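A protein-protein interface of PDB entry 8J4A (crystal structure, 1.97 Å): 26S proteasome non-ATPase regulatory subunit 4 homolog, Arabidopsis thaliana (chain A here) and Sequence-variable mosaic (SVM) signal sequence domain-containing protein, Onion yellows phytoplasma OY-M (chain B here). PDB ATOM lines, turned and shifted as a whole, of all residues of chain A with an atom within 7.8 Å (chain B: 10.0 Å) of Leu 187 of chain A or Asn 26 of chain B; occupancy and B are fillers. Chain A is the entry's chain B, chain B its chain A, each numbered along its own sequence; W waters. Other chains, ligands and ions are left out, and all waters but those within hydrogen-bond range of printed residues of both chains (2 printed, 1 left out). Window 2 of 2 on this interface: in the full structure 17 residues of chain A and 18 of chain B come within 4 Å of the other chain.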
ATOM      1  N   ALA A  33     -23.515   4.000  22.679  1.00  0.00           N
ATOM      2  CA  ALA A  33     -22.687   4.795  21.772  1.00  0.00           C
ATOM      3  C   ALA A  33     -23.357   6.117  21.438  1.00  0.00           C
ATOM      4  O   ALA A  33     -22.715   7.174  21.449  1.00  0.00           O
ATOM      5  CB  ALA A  33     -22.405   4.021  20.483  1.00  0.00           C
ATOM      6  N   ASN A  35     -25.737   7.755  23.073  1.00  0.00           N
ATOM      7  CA  ASN A  35     -25.773   8.646  24.226  1.00  0.00           C
ATOM      8  C   ASN A  35     -24.426   9.335  24.427  1.00  0.00           C
ATOM      9  O   ASN A  35     -24.366  10.553  24.602  1.00  0.00           O
ATOM     10  CB  ASN A  35     -26.196   7.875  25.474  1.00  0.00           C
ATOM     11  CG  ASN A  35     -27.667   7.523  25.452  1.00  0.00           C
ATOM     12  OD1 ASN A  35     -28.456   8.167  24.766  1.00  0.00           O
ATOM     13  ND2 ASN A  35     -28.036   6.477  26.170  1.00  0.00           N
ATOM     14  N   LEU A  36     -23.327   8.572  24.366  1.00  0.00           N
ATOM     15  CA  LEU A  36     -22.000   9.177  24.535  1.00  0.00           C
ATOM     16  C   LEU A  36     -21.716  10.212  23.456  1.00  0.00           C
ATOM     17  O   LEU A  36     -21.142  11.270  23.734  1.00  0.00           O
ATOM     18  CB  LEU A  36     -20.921   8.097  24.518  1.00  0.00           C
ATOM     19  CG  LEU A  36     -20.950   7.112  25.693  1.00  0.00           C
ATOM     20  CD1 LEU A  36     -19.681   6.256  25.743  1.00  0.00           C
ATOM     21  CD2 LEU A  36     -21.125   7.879  26.990  1.00  0.00           C
ATOM     22  N   LEU A  37     -22.094   9.908  22.208  1.00  0.00           N
ATOM     23  CA  LEU A  37     -21.866  10.834  21.099  1.00  0.00           C
ATOM     24  C   LEU A  37     -22.644  12.127  21.299  1.00  0.00           C
ATOM     25  O   LEU A  37     -22.099  13.225  21.126  1.00  0.00           O
ATOM     26  CB  LEU A  37     -22.256  10.152  19.779  1.00  0.00           C
ATOM     27  CG  LEU A  37     -21.792  10.699  18.434  1.00  0.00           C
ATOM     28  CD1 LEU A  37     -20.296  10.915  18.403  1.00  0.00           C
ATOM     29  CD2 LEU A  37     -22.195   9.750  17.322  1.00  0.00           C
ATOM     30  N   GLY A  39     -23.609  13.463  24.118  1.00  0.00           N
ATOM     31  CA  GLY A  39     -22.935  14.222  25.156  1.00  0.00           C
ATOM     32  C   GLY A  39     -21.671  14.885  24.645  1.00  0.00           C
ATOM     33  O   GLY A  39     -21.420  16.056  24.920  1.00  0.00           O
ATOM     34  N   ALA A  40     -20.875  14.154  23.864  1.00  0.00           N
ATOM     35  CA  ALA A  40     -19.606  14.700  23.395  1.00  0.00           C
ATOM     36  C   ALA A  40     -19.829  15.888  22.459  1.00  0.00           C
ATOM     37  O   ALA A  40     -19.193  16.938  22.608  1.00  0.00           O
ATOM     38  CB  ALA A  40     -18.799  13.603  22.705  1.00  0.00           C
ATOM     39  N   VAL A 173     -16.041   3.204  10.260  1.00  0.00           N
ATOM     40  CA  VAL A 173     -15.488   2.333  11.287  1.00  0.00           C
ATOM     41  C   VAL A 173     -16.148   0.974  11.133  1.00  0.00           C
ATOM     42  O   VAL A 173     -17.381   0.882  11.122  1.00  0.00           O
ATOM     43  CB  VAL A 173     -15.701   2.873  12.714  1.00  0.00           C
ATOM     44  CG1 VAL A 173     -14.895   2.044  13.718  1.00  0.00           C
ATOM     45  CG2 VAL A 173     -15.322   4.349  12.819  1.00  0.00           C
ATOM     46  N   ASN A 180     -13.781  -5.296  23.107  1.00  0.00           N
ATOM     47  CA  ASN A 180     -14.154  -3.915  23.361  1.00  0.00           C
ATOM     48  C   ASN A 180     -15.525  -3.622  22.768  1.00  0.00           C
ATOM     49  O   ASN A 180     -15.778  -3.886  21.588  1.00  0.00           O
ATOM     50  CB  ASN A 180     -13.104  -2.955  22.810  1.00  0.00           C
ATOM     51  CG  ASN A 180     -12.113  -2.521  23.879  1.00  0.00           C
ATOM     52  OD1 ASN A 180     -12.206  -1.415  24.424  1.00  0.00           O
ATOM     53  ND2 ASN A 180     -11.174  -3.402  24.203  1.00  0.00           N
ATOM     54  N   ALA A 181     -16.406  -3.088  23.608  1.00  0.00           N
ATOM     55  CA  ALA A 181     -17.758  -2.761  23.204  1.00  0.00           C
ATOM     56  C   ALA A 181     -17.754  -1.705  22.098  1.00  0.00           C
ATOM     57  O   ALA A 181     -16.771  -0.990  21.878  1.00  0.00           O
ATOM     58  CB  ALA A 181     -18.553  -2.272  24.413  1.00  0.00           C
ATOM     59  N   LEU A 182     -18.883  -1.625  21.394  1.00  0.00           N
ATOM     60  CA  LEU A 182     -19.049  -0.652  20.319  1.00  0.00           C
ATOM     61  C   LEU A 182     -18.584   0.740  20.741  1.00  0.00           C
ATOM     62  O   LEU A 182     -17.768   1.371  20.061  1.00  0.00           O
ATOM     63  CB  LEU A 182     -20.516  -0.631  19.892  1.00  0.00           C
ATOM     64  CG  LEU A 182     -20.950   0.170  18.671  1.00  0.00           C
ATOM     65  CD1 LEU A 182     -20.721  -0.664  17.458  1.00  0.00           C
ATOM     66  CD2 LEU A 182     -22.416   0.536  18.746  1.00  0.00           C
ATOM     67  N   SER A 183     -19.082   1.225  21.883  1.00  0.00           N
ATOM     68  CA  SER A 183     -18.762   2.582  22.315  1.00  0.00           C
ATOM     69  C   SER A 183     -17.265   2.751  22.543  1.00  0.00           C
ATOM     70  O   SER A 183     -16.679   3.762  22.133  1.00  0.00           O
ATOM     71  CB  SER A 183     -19.567   2.936  23.574  1.00  0.00           C
ATOM     72  OG  SER A 183     -18.903   2.520  24.758  1.00  0.00           O
ATOM     73  N   ASP A 184     -16.615   1.750  23.143  1.00  0.00           N
ATOM     74  CA  ASP A 184     -15.189   1.857  23.422  1.00  0.00           C
ATOM     75  C   ASP A 184     -14.387   1.980  22.134  1.00  0.00           C
ATOM     76  O   ASP A 184     -13.504   2.837  22.020  1.00  0.00           O
ATOM     77  CB  ASP A 184     -14.720   0.654  24.239  1.00  0.00           C
ATOM     78  CG  ASP A 184     -15.114   0.759  25.694  1.00  0.00           C
ATOM     79  OD1 ASP A 184     -15.735   1.787  26.062  1.00  0.00           O
ATOM     80  OD2 ASP A 184     -14.806  -0.177  26.467  1.00  0.00           O
ATOM     81  N   VAL A 185     -14.696   1.143  21.144  1.00  0.00           N
ATOM     82  CA  VAL A 185     -14.031   1.244  19.845  1.00  0.00           C
ATOM     83  C   VAL A 185     -14.215   2.640  19.248  1.00  0.00           C
ATOM     84  O   VAL A 185     -13.260   3.263  18.768  1.00  0.00           O
ATOM     85  CB  VAL A 185     -14.547   0.145  18.897  1.00  0.00           C
ATOM     86  CG1 VAL A 185     -13.820   0.223  17.547  1.00  0.00           C
ATOM     87  CG2 VAL A 185     -14.366  -1.233  19.536  1.00  0.00           C
ATOM     88  N   LEU A 186     -15.442   3.168  19.304  1.00  0.00           N
ATOM     89  CA  LEU A 186     -15.743   4.444  18.663  1.00  0.00           C
ATOM     90  C   LEU A 186     -15.031   5.622  19.317  1.00  0.00           C
ATOM     91  O   LEU A 186     -14.736   6.613  18.633  1.00  0.00           O
ATOM     92  CB  LEU A 186     -17.257   4.687  18.670  1.00  0.00           C
ATOM     93  CG  LEU A 186     -18.060   3.746  17.766  1.00  0.00           C
ATOM     94  CD1 LEU A 186     -19.525   4.133  17.730  1.00  0.00           C
ATOM     95  CD2 LEU A 186     -17.459   3.717  16.334  1.00  0.00           C
ATOM     96  N   LEU A 187     -14.777   5.556  20.627  1.00  0.00           N
ATOM     97  CA  LEU A 187     -14.280   6.719  21.357  1.00  0.00           C
ATOM     98  C   LEU A 187     -12.943   7.199  20.813  1.00  0.00           C
ATOM     99  O   LEU A 187     -12.670   8.411  20.806  1.00  0.00           O
ATOM    100  CB  LEU A 187     -14.152   6.394  22.851  1.00  0.00           C
ATOM    101  CG  LEU A 187     -15.437   6.346  23.681  1.00  0.00           C
ATOM    102  CD1 LEU A 187     -15.242   5.571  24.975  1.00  0.00           C
ATOM    103  CD2 LEU A 187     -15.938   7.749  23.962  1.00  0.00           C
ATOM    104  N   SER A 188     -12.106   6.278  20.340  1.00  0.00           N
ATOM    105  CA  SER A 188     -10.780   6.623  19.843  1.00  0.00           C
ATOM    106  C   SER A 188     -10.739   6.873  18.333  1.00  0.00           C
ATOM    107  O   SER A 188      -9.643   6.959  17.771  1.00  0.00           O
ATOM    108  CB  SER A 188      -9.776   5.522  20.213  1.00  0.00           C
ATOM    109  OG  SER A 188     -10.167   4.280  19.657  1.00  0.00           O
ATOM    110  N   THR A 189     -11.886   6.990  17.669  1.00  0.00           N
ATOM    111  CA  THR A 189     -11.960   7.223  16.233  1.00  0.00           C
ATOM    112  C   THR A 189     -12.455   8.633  15.934  1.00  0.00           C
ATOM    113  O   THR A 189     -12.937   9.343  16.824  1.00  0.00           O
ATOM    114  CB  THR A 189     -12.882   6.195  15.553  1.00  0.00           C
ATOM    115  OG1 THR A 189     -14.252   6.515  15.839  1.00  0.00           O
ATOM    116  CG2 THR A 189     -12.559   4.772  16.001  1.00  0.00           C
ATOM    117  N   PRO A 190     -12.336   9.084  14.680  1.00  0.00           N
ATOM    118  CA  PRO A 190     -12.822  10.428  14.338  1.00  0.00           C
ATOM    119  C   PRO A 190     -14.320  10.605  14.491  1.00  0.00           C
ATOM    120  O   PRO A 190     -14.802  11.739  14.368  1.00  0.00           O
ATOM    121  CB  PRO A 190     -12.393  10.589  12.873  1.00  0.00           C
ATOM    122  CG  PRO A 190     -11.187   9.705  12.751  1.00  0.00           C
ATOM    123  CD  PRO A 190     -11.514   8.515  13.592  1.00  0.00           C
ATOM    124  N   VAL A 191     -15.084   9.538  14.723  1.00  0.00           N
ATOM    125  CA  VAL A 191     -16.497   9.741  15.036  1.00  0.00           C
ATOM    126  C   VAL A 191     -16.631  10.626  16.266  1.00  0.00           C
ATOM    127  O   VAL A 191     -17.504  11.507  16.328  1.00  0.00           O
ATOM    128  CB  VAL A 191     -17.217   8.397  15.237  1.00  0.00           C
ATOM    129  CG1 VAL A 191     -18.697   8.634  15.532  1.00  0.00           C
ATOM    130  CG2 VAL A 191     -17.048   7.514  14.025  1.00  0.00           C
ATOM    131  N   PHE A 192     -15.761  10.413  17.258  1.00  0.00           N
ATOM    132  CA  PHE A 192     -15.709  11.218  18.476  1.00  0.00           C
ATOM    133  C   PHE A 192     -14.622  12.285  18.441  1.00  0.00           C
ATOM    134  O   PHE A 192     -14.837  13.396  18.936  1.00  0.00           O
ATOM    135  CB  PHE A 192     -15.462  10.326  19.697  1.00  0.00           C
ATOM    136  CG  PHE A 192     -16.692   9.673  20.232  1.00  0.00           C
ATOM    137  CD1 PHE A 192     -17.177   8.502  19.664  1.00  0.00           C
ATOM    138  CD2 PHE A 192     -17.365  10.223  21.310  1.00  0.00           C
ATOM    139  CE1 PHE A 192     -18.323   7.885  20.171  1.00  0.00           C
ATOM    140  CE2 PHE A 192     -18.506   9.610  21.819  1.00  0.00           C
ATOM    141  CZ  PHE A 192     -18.987   8.449  21.250  1.00  0.00           C
ATOM    142  N   THR A 193     -13.463  11.953  17.876  1.00  0.00           N
ATOM    143  CA  THR A 193     -12.306  12.845  17.793  1.00  0.00           C
ATOM    144  C   THR A 193     -12.180  13.449  16.398  1.00  0.00           C
ATOM    145  O   THR A 193     -11.136  13.322  15.755  1.00  0.00           O
ATOM    146  CB  THR A 193     -11.029  12.085  18.110  1.00  0.00           C
ATOM    147  OG1 THR A 193     -10.658  11.354  16.934  1.00  0.00           O
ATOM    148  CG2 THR A 193     -11.245  11.117  19.261  1.00  0.00           C
ATOM    149  N   GLY A 194     -13.253  14.085  15.925  1.00  0.00           N
ATOM    150  CA  GLY A 194     -13.249  14.768  14.633  1.00  0.00           C
ATOM    151  C   GLY A 194     -12.543  14.045  13.497  1.00  0.00           C
ATOM    152  O   GLY A 194     -12.133  14.657  12.506  1.00  0.00           O
ATOM    153  N   PHE B  18     -26.980   1.991  31.110  1.00  0.00           N
ATOM    154  CA  PHE B  18     -25.666   1.524  30.693  1.00  0.00           C
ATOM    155  C   PHE B  18     -25.405   0.137  31.265  1.00  0.00           C
ATOM    156  O   PHE B  18     -25.798  -0.164  32.392  1.00  0.00           O
ATOM    157  CB  PHE B  18     -24.555   2.469  31.188  1.00  0.00           C
ATOM    158  CG  PHE B  18     -24.445   3.760  30.413  1.00  0.00           C
ATOM    159  CD1 PHE B  18     -23.863   3.781  29.159  1.00  0.00           C
ATOM    160  CD2 PHE B  18     -24.870   4.951  30.967  1.00  0.00           C
ATOM    161  CE1 PHE B  18     -23.730   4.958  28.457  1.00  0.00           C
ATOM    162  CE2 PHE B  18     -24.739   6.133  30.276  1.00  0.00           C
ATOM    163  CZ  PHE B  18     -24.178   6.136  29.012  1.00  0.00           C
ATOM    164  N   ASP B  20     -22.504  -0.847  32.145  1.00  0.00           N
ATOM    165  CA  ASP B  20     -21.343  -0.724  33.017  1.00  0.00           C
ATOM    166  C   ASP B  20     -21.265   0.706  33.517  1.00  0.00           C
ATOM    167  O   ASP B  20     -21.235   1.639  32.709  1.00  0.00           O
ATOM    168  CB  ASP B  20     -20.070  -1.095  32.257  1.00  0.00           C
ATOM    169  CG  ASP B  20     -18.945  -1.496  33.174  1.00  0.00           C
ATOM    170  OD1 ASP B  20     -18.525  -0.653  33.999  1.00  0.00           O
ATOM    171  OD2 ASP B  20     -18.471  -2.653  33.064  1.00  0.00           O
ATOM    172  N   ILE B  21     -21.226   0.874  34.843  1.00  0.00           N
ATOM    173  CA  ILE B  21     -21.075   2.203  35.433  1.00  0.00           C
ATOM    174  C   ILE B  21     -19.869   2.934  34.855  1.00  0.00           C
ATOM    175  O   ILE B  21     -19.888   4.163  34.705  1.00  0.00           O
ATOM    176  CB  ILE B  21     -20.971   2.096  36.967  1.00  0.00           C
ATOM    177  CG1 ILE B  21     -20.803   3.486  37.583  1.00  0.00           C
ATOM    178  CG2 ILE B  21     -19.788   1.234  37.360  1.00  0.00           C
ATOM    179  CD1 ILE B  21     -22.089   4.241  37.768  1.00  0.00           C
ATOM    180  N   ASN B  22     -18.810   2.202  34.512  1.00  0.00           N
ATOM    181  CA  ASN B  22     -17.597   2.871  34.036  1.00  0.00           C
ATOM    182  C   ASN B  22     -17.796   3.552  32.684  1.00  0.00           C
ATOM    183  O   ASN B  22     -17.051   4.483  32.353  1.00  0.00           O
ATOM    184  CB  ASN B  22     -16.433   1.873  33.960  1.00  0.00           C
ATOM    185  CG  ASN B  22     -15.755   1.641  35.317  1.00  0.00           C
ATOM    186  OD1 ASN B  22     -15.745   2.518  36.183  1.00  0.00           O
ATOM    187  ND2 ASN B  22     -15.184   0.451  35.499  1.00  0.00           N
ATOM    188  N   SER B  23     -18.780   3.121  31.890  1.00  0.00           N
ATOM    189  CA  SER B  23     -19.058   3.844  30.652  1.00  0.00           C
ATOM    190  C   SER B  23     -19.452   5.282  30.937  1.00  0.00           C
ATOM    191  O   SER B  23     -19.241   6.169  30.105  1.00  0.00           O
ATOM    192  CB  SER B  23     -20.157   3.155  29.843  1.00  0.00           C
ATOM    193  OG  SER B  23     -19.718   1.903  29.347  1.00  0.00           O
ATOM    194  N   ILE B  24     -20.014   5.543  32.113  1.00  0.00           N
ATOM    195  CA  ILE B  24     -20.407   6.900  32.453  1.00  0.00           C
ATOM    196  C   ILE B  24     -19.199   7.820  32.590  1.00  0.00           C
ATOM    197  O   ILE B  24     -19.335   9.039  32.430  1.00  0.00           O
ATOM    198  CB  ILE B  24     -21.255   6.885  33.731  1.00  0.00           C
ATOM    199  CG1 ILE B  24     -22.565   6.140  33.478  1.00  0.00           C
ATOM    200  CG2 ILE B  24     -21.597   8.300  34.174  1.00  0.00           C
ATOM    201  CD1 ILE B  24     -23.488   6.176  34.698  1.00  0.00           C
ATOM    202  N   LYS B  25     -18.013   7.265  32.859  1.00  0.00           N
ATOM    203  CA  LYS B  25     -16.816   8.086  32.999  1.00  0.00           C
ATOM    204  C   LYS B  25     -16.423   8.786  31.704  1.00  0.00           C
ATOM    205  O   LYS B  25     -15.657   9.751  31.750  1.00  0.00           O
ATOM    206  CB  LYS B  25     -15.658   7.233  33.512  1.00  0.00           C
ATOM    207  CG  LYS B  25     -15.830   6.802  34.978  1.00  0.00           C
ATOM    208  CD  LYS B  25     -14.943   5.618  35.326  1.00  0.00           C
ATOM    209  CE  LYS B  25     -14.718   5.510  36.836  1.00  0.00           C
ATOM    210  NZ  LYS B  25     -14.070   4.217  37.268  1.00  0.00           N
ATOM    211  N   ASN B  26     -16.914   8.328  30.555  1.00  0.00           N
ATOM    212  CA  ASN B  26     -16.677   9.003  29.282  1.00  0.00           C
ATOM    213  C   ASN B  26     -17.901   9.759  28.790  1.00  0.00           C
ATOM    214  O   ASN B  26     -17.938  10.179  27.626  1.00  0.00           O
ATOM    215  CB  ASN B  26     -16.255   8.004  28.216  1.00  0.00           C
ATOM    216  CG  ASN B  26     -14.856   7.494  28.426  1.00  0.00           C
ATOM    217  OD1 ASN B  26     -14.650   6.299  28.617  1.00  0.00           O
ATOM    218  ND2 ASN B  26     -13.879   8.396  28.367  1.00  0.00           N
ATOM    219  N   PHE B  27     -18.903   9.932  29.643  1.00  0.00           N
ATOM    220  CA  PHE B  27     -20.190  10.503  29.245  1.00  0.00           C
ATOM    221  C   PHE B  27     -20.196  11.964  29.680  1.00  0.00           C
ATOM    222  O   PHE B  27     -20.443  12.272  30.849  1.00  0.00           O
ATOM    223  CB  PHE B  27     -21.323   9.700  29.870  1.00  0.00           C
ATOM    224  CG  PHE B  27     -22.691  10.046  29.356  1.00  0.00           C
ATOM    225  CD1 PHE B  27     -22.856  10.837  28.229  1.00  0.00           C
ATOM    226  CD2 PHE B  27     -23.825   9.563  30.008  1.00  0.00           C
ATOM    227  CE1 PHE B  27     -24.132  11.157  27.767  1.00  0.00           C
ATOM    228  CE2 PHE B  27     -25.112   9.869  29.541  1.00  0.00           C
ATOM    229  CZ  PHE B  27     -25.260  10.661  28.420  1.00  0.00           C
ATOM    230  N   GLN B  28     -19.892  12.881  28.722  1.00  0.00           N
ATOM    231  CA  GLN B  28     -19.912  14.312  28.999  1.00  0.00           C
ATOM    232  C   GLN B  28     -21.348  14.828  29.029  1.00  0.00           C
ATOM    233  O   GLN B  28     -22.175  14.411  28.213  1.00  0.00           O
ATOM    234  CB  GLN B  28     -19.124  15.073  27.941  1.00  0.00           C
ATOM    235  CG  GLN B  28     -17.804  14.442  27.592  1.00  0.00           C
ATOM    236  CD  GLN B  28     -17.022  15.294  26.627  1.00  0.00           C
ATOM    237  OE1 GLN B  28     -16.938  16.516  26.790  1.00  0.00           O
ATOM    238  NE2 GLN B  28     -16.456  14.665  25.604  1.00  0.00           N
ATOM    239  N   PRO B  29     -21.682  15.721  29.968  1.00  0.00           N
ATOM    240  CA  PRO B  29     -20.873  16.294  31.047  1.00  0.00           C
ATOM    241  C   PRO B  29     -20.990  15.539  32.368  1.00  0.00           C
ATOM    242  O   PRO B  29     -20.397  15.931  33.371  1.00  0.00           O
ATOM    243  CB  PRO B  29     -21.461  17.696  31.189  1.00  0.00           C
ATOM    244  CG  PRO B  29     -22.907  17.487  30.910  1.00  0.00           C
ATOM    245  CD  PRO B  29     -23.026  16.322  29.936  1.00  0.00           C
ATOM    246  N   PHE B  30     -21.757  14.450  32.343  1.00  0.00           N
ATOM    247  CA  PHE B  30     -22.124  13.749  33.565  1.00  0.00           C
ATOM    248  C   PHE B  30     -20.934  13.138  34.276  1.00  0.00           C
ATOM    249  O   PHE B  30     -20.988  12.941  35.494  1.00  0.00           O
ATOM    250  CB  PHE B  30     -23.136  12.673  33.222  1.00  0.00           C
ATOM    251  CG  PHE B  30     -24.323  13.214  32.498  1.00  0.00           C
ATOM    252  CD1 PHE B  30     -25.139  14.147  33.106  1.00  0.00           C
ATOM    253  CD2 PHE B  30     -24.621  12.801  31.228  1.00  0.00           C
ATOM    254  CE1 PHE B  30     -26.242  14.650  32.449  1.00  0.00           C
ATOM    255  CE2 PHE B  30     -25.730  13.304  30.577  1.00  0.00           C
ATOM    256  CZ  PHE B  30     -26.517  14.232  31.185  1.00  0.00           C
ATOM    257  N   SER B  31     -19.874  12.803  33.543  1.00  0.00           N
ATOM    258  CA  SER B  31     -18.675  12.289  34.199  1.00  0.00           C
ATOM    259  C   SER B  31     -18.089  13.274  35.212  1.00  0.00           C
ATOM    260  O   SER B  31     -17.368  12.844  36.123  1.00  0.00           O
ATOM    261  CB  SER B  31     -17.631  11.907  33.147  1.00  0.00           C
ATOM    262  OG  SER B  31     -17.327  13.004  32.309  1.00  0.00           O
ATOM    263  N   GLN B  32     -18.402  14.577  35.100  1.00  0.00           N
ATOM    264  CA  GLN B  32     -17.899  15.577  36.039  1.00  0.00           C
ATOM    265  C   GLN B  32     -18.756  15.731  37.288  1.00  0.00           C
ATOM    266  O   GLN B  32     -18.314  16.383  38.240  1.00  0.00           O
ATOM    267  CB  GLN B  32     -17.787  16.951  35.374  1.00  0.00           C
ATOM    268  CG  GLN B  32     -16.839  17.008  34.205  1.00  0.00           C
ATOM    269  CD  GLN B  32     -15.370  16.982  34.594  1.00  0.00           C
ATOM    270  OE1 GLN B  32     -14.999  16.607  35.716  1.00  0.00           O
ATOM    271  NE2 GLN B  32     -14.515  17.395  33.654  1.00  0.00           N
ATOM    272  N   PHE B  34     -20.811  12.888  38.697  1.00  0.00           N
ATOM    273  CA  PHE B  34     -20.712  11.665  39.475  1.00  0.00           C
ATOM    274  C   PHE B  34     -19.485  11.745  40.378  1.00  0.00           C
ATOM    275  O   PHE B  34     -18.489  12.398  40.051  1.00  0.00           O
ATOM    276  CB  PHE B  34     -20.581  10.457  38.542  1.00  0.00           C
ATOM    277  CG  PHE B  34     -21.880   9.755  38.242  1.00  0.00           C
ATOM    278  CD1 PHE B  34     -22.740  10.236  37.253  1.00  0.00           C
ATOM    279  CD2 PHE B  34     -22.217   8.585  38.911  1.00  0.00           C
ATOM    280  CE1 PHE B  34     -23.922   9.578  36.959  1.00  0.00           C
ATOM    281  CE2 PHE B  34     -23.402   7.902  38.619  1.00  0.00           C
ATOM    282  CZ  PHE B  34     -24.261   8.413  37.640  1.00  0.00           C
ATOM    283  N   PHE B  36     -17.319   8.855  41.497  1.00  0.00           N
ATOM    284  CA  PHE B  36     -17.222   7.410  41.338  1.00  0.00           C
ATOM    285  C   PHE B  36     -16.476   6.727  42.474  1.00  0.00           C
ATOM    286  O   PHE B  36     -16.385   5.494  42.455  1.00  0.00           O
ATOM    287  CB  PHE B  36     -16.551   7.067  40.009  1.00  0.00           C
ATOM    288  CG  PHE B  36     -17.316   7.540  38.796  1.00  0.00           C
ATOM    289  CD1 PHE B  36     -18.403   6.830  38.328  1.00  0.00           C
ATOM    290  CD2 PHE B  36     -16.935   8.691  38.121  1.00  0.00           C
ATOM    291  CE1 PHE B  36     -19.105   7.259  37.195  1.00  0.00           C
ATOM    292  CE2 PHE B  36     -17.629   9.126  37.004  1.00  0.00           C
ATOM    293  CZ  PHE B  36     -18.714   8.407  36.537  1.00  0.00           C
ATOM    294  N   PHE B  98     -29.853   7.448  36.116  1.00  0.00           N
ATOM    295  CA  PHE B  98     -28.916   6.533  35.478  1.00  0.00           C
ATOM    296  C   PHE B  98     -29.140   5.141  36.027  1.00  0.00           C
ATOM    297  O   PHE B  98     -29.142   4.955  37.248  1.00  0.00           O
ATOM    298  CB  PHE B  98     -27.470   6.947  35.728  1.00  0.00           C
ATOM    299  CG  PHE B  98     -27.120   8.276  35.148  1.00  0.00           C
ATOM    300  CD1 PHE B  98     -27.391   9.448  35.841  1.00  0.00           C
ATOM    301  CD2 PHE B  98     -26.512   8.351  33.912  1.00  0.00           C
ATOM    302  CE1 PHE B  98     -27.083  10.690  35.275  1.00  0.00           C
ATOM    303  CE2 PHE B  98     -26.184   9.574  33.361  1.00  0.00           C
ATOM    304  CZ  PHE B  98     -26.468  10.745  34.050  1.00  0.00           C
HETATM  305  O   HOH W   1     -19.674  11.868  25.963  1.00  0.00           O
HETATM  306  O   HOH W   2     -16.813  17.228  23.666  1.00  0.00           O
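Among the printed residues, pairs that only touch across the chains: Gly 39 of chain A with Gln 28 of chain B (3.2 Å), Asn 35 of chain A with Phe 27 of chain B (3.2 Å), Leu 36 of chain A with Phe 27 of chain B (3.4 Å), Leu 187 of chain A with Asn 26 of chain B (3.8 Å), Ala 40 of chain A with Gln 28 of chain B (3.8 Å) and Leu 36 of chain A with Asn 26 of chain B (3.98 Å).
Hydrophobic or aromatic side chains of chain A that line the printed part of chain B: Leu 36, Ala 40 and Leu 187. Among the printed residues, 6 pairs touch across the chains.
Water W2 lies within hydrogen-bond range of O of Ala 40 of chain A (2.6 Å) and OE1 of Gln 28 of chain B (3.2 Å). Water W1 lies within hydrogen-bond range of O of Leu 36 of chain A (2.7 Å), O of Asn 26 of chain B (2.9 Å), N of Gln 28 of chain B (2.9 Å) and N of Ala 40 of chain A (3.3 Å).
Of chain B, only Asn 26 (3.8 Å) comes within 4 Å of Leu 187 of chain A. Of the printed residues of chain A, Asn 26 of chain B touches Leu 36 and Leu 187. No residue of chain B comes within 4 Å of Leu 186 of chain A. No residue of chain B comes within 4 Å of Ser 188 of chain A. No residue of chain B comes within 4 Å of Phe 192 of chain A. Printed residues of chain B within 4 Å of Ala 40 of chain A: Gln 28. Printed residues of chain A within 4 Å of Gln 28 of chain B: Gly 39 (3.2 Å) and Ala 40 (3.8 Å). Printed residues of chain B within 4 Å of Leu 36 of chain A: Asn 26 and Phe 27. Gln 32 of chain B touches none of the printed residues of chain A. Phe 34 of chain B touches none of the printed residues of chain A. The nearest residue of chain B that does not touch Leu 187 of chain A is Ser 23 of chain B (6.5 Å). The nearest printed residue of chain A that does not touch Asn 26 of chain B is Asp 184 of chain A (5.3 Å). The nearest printed residue of chain B that does not touch Ala 40 of chain A is Phe 27 of chain B (5.8 Å).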
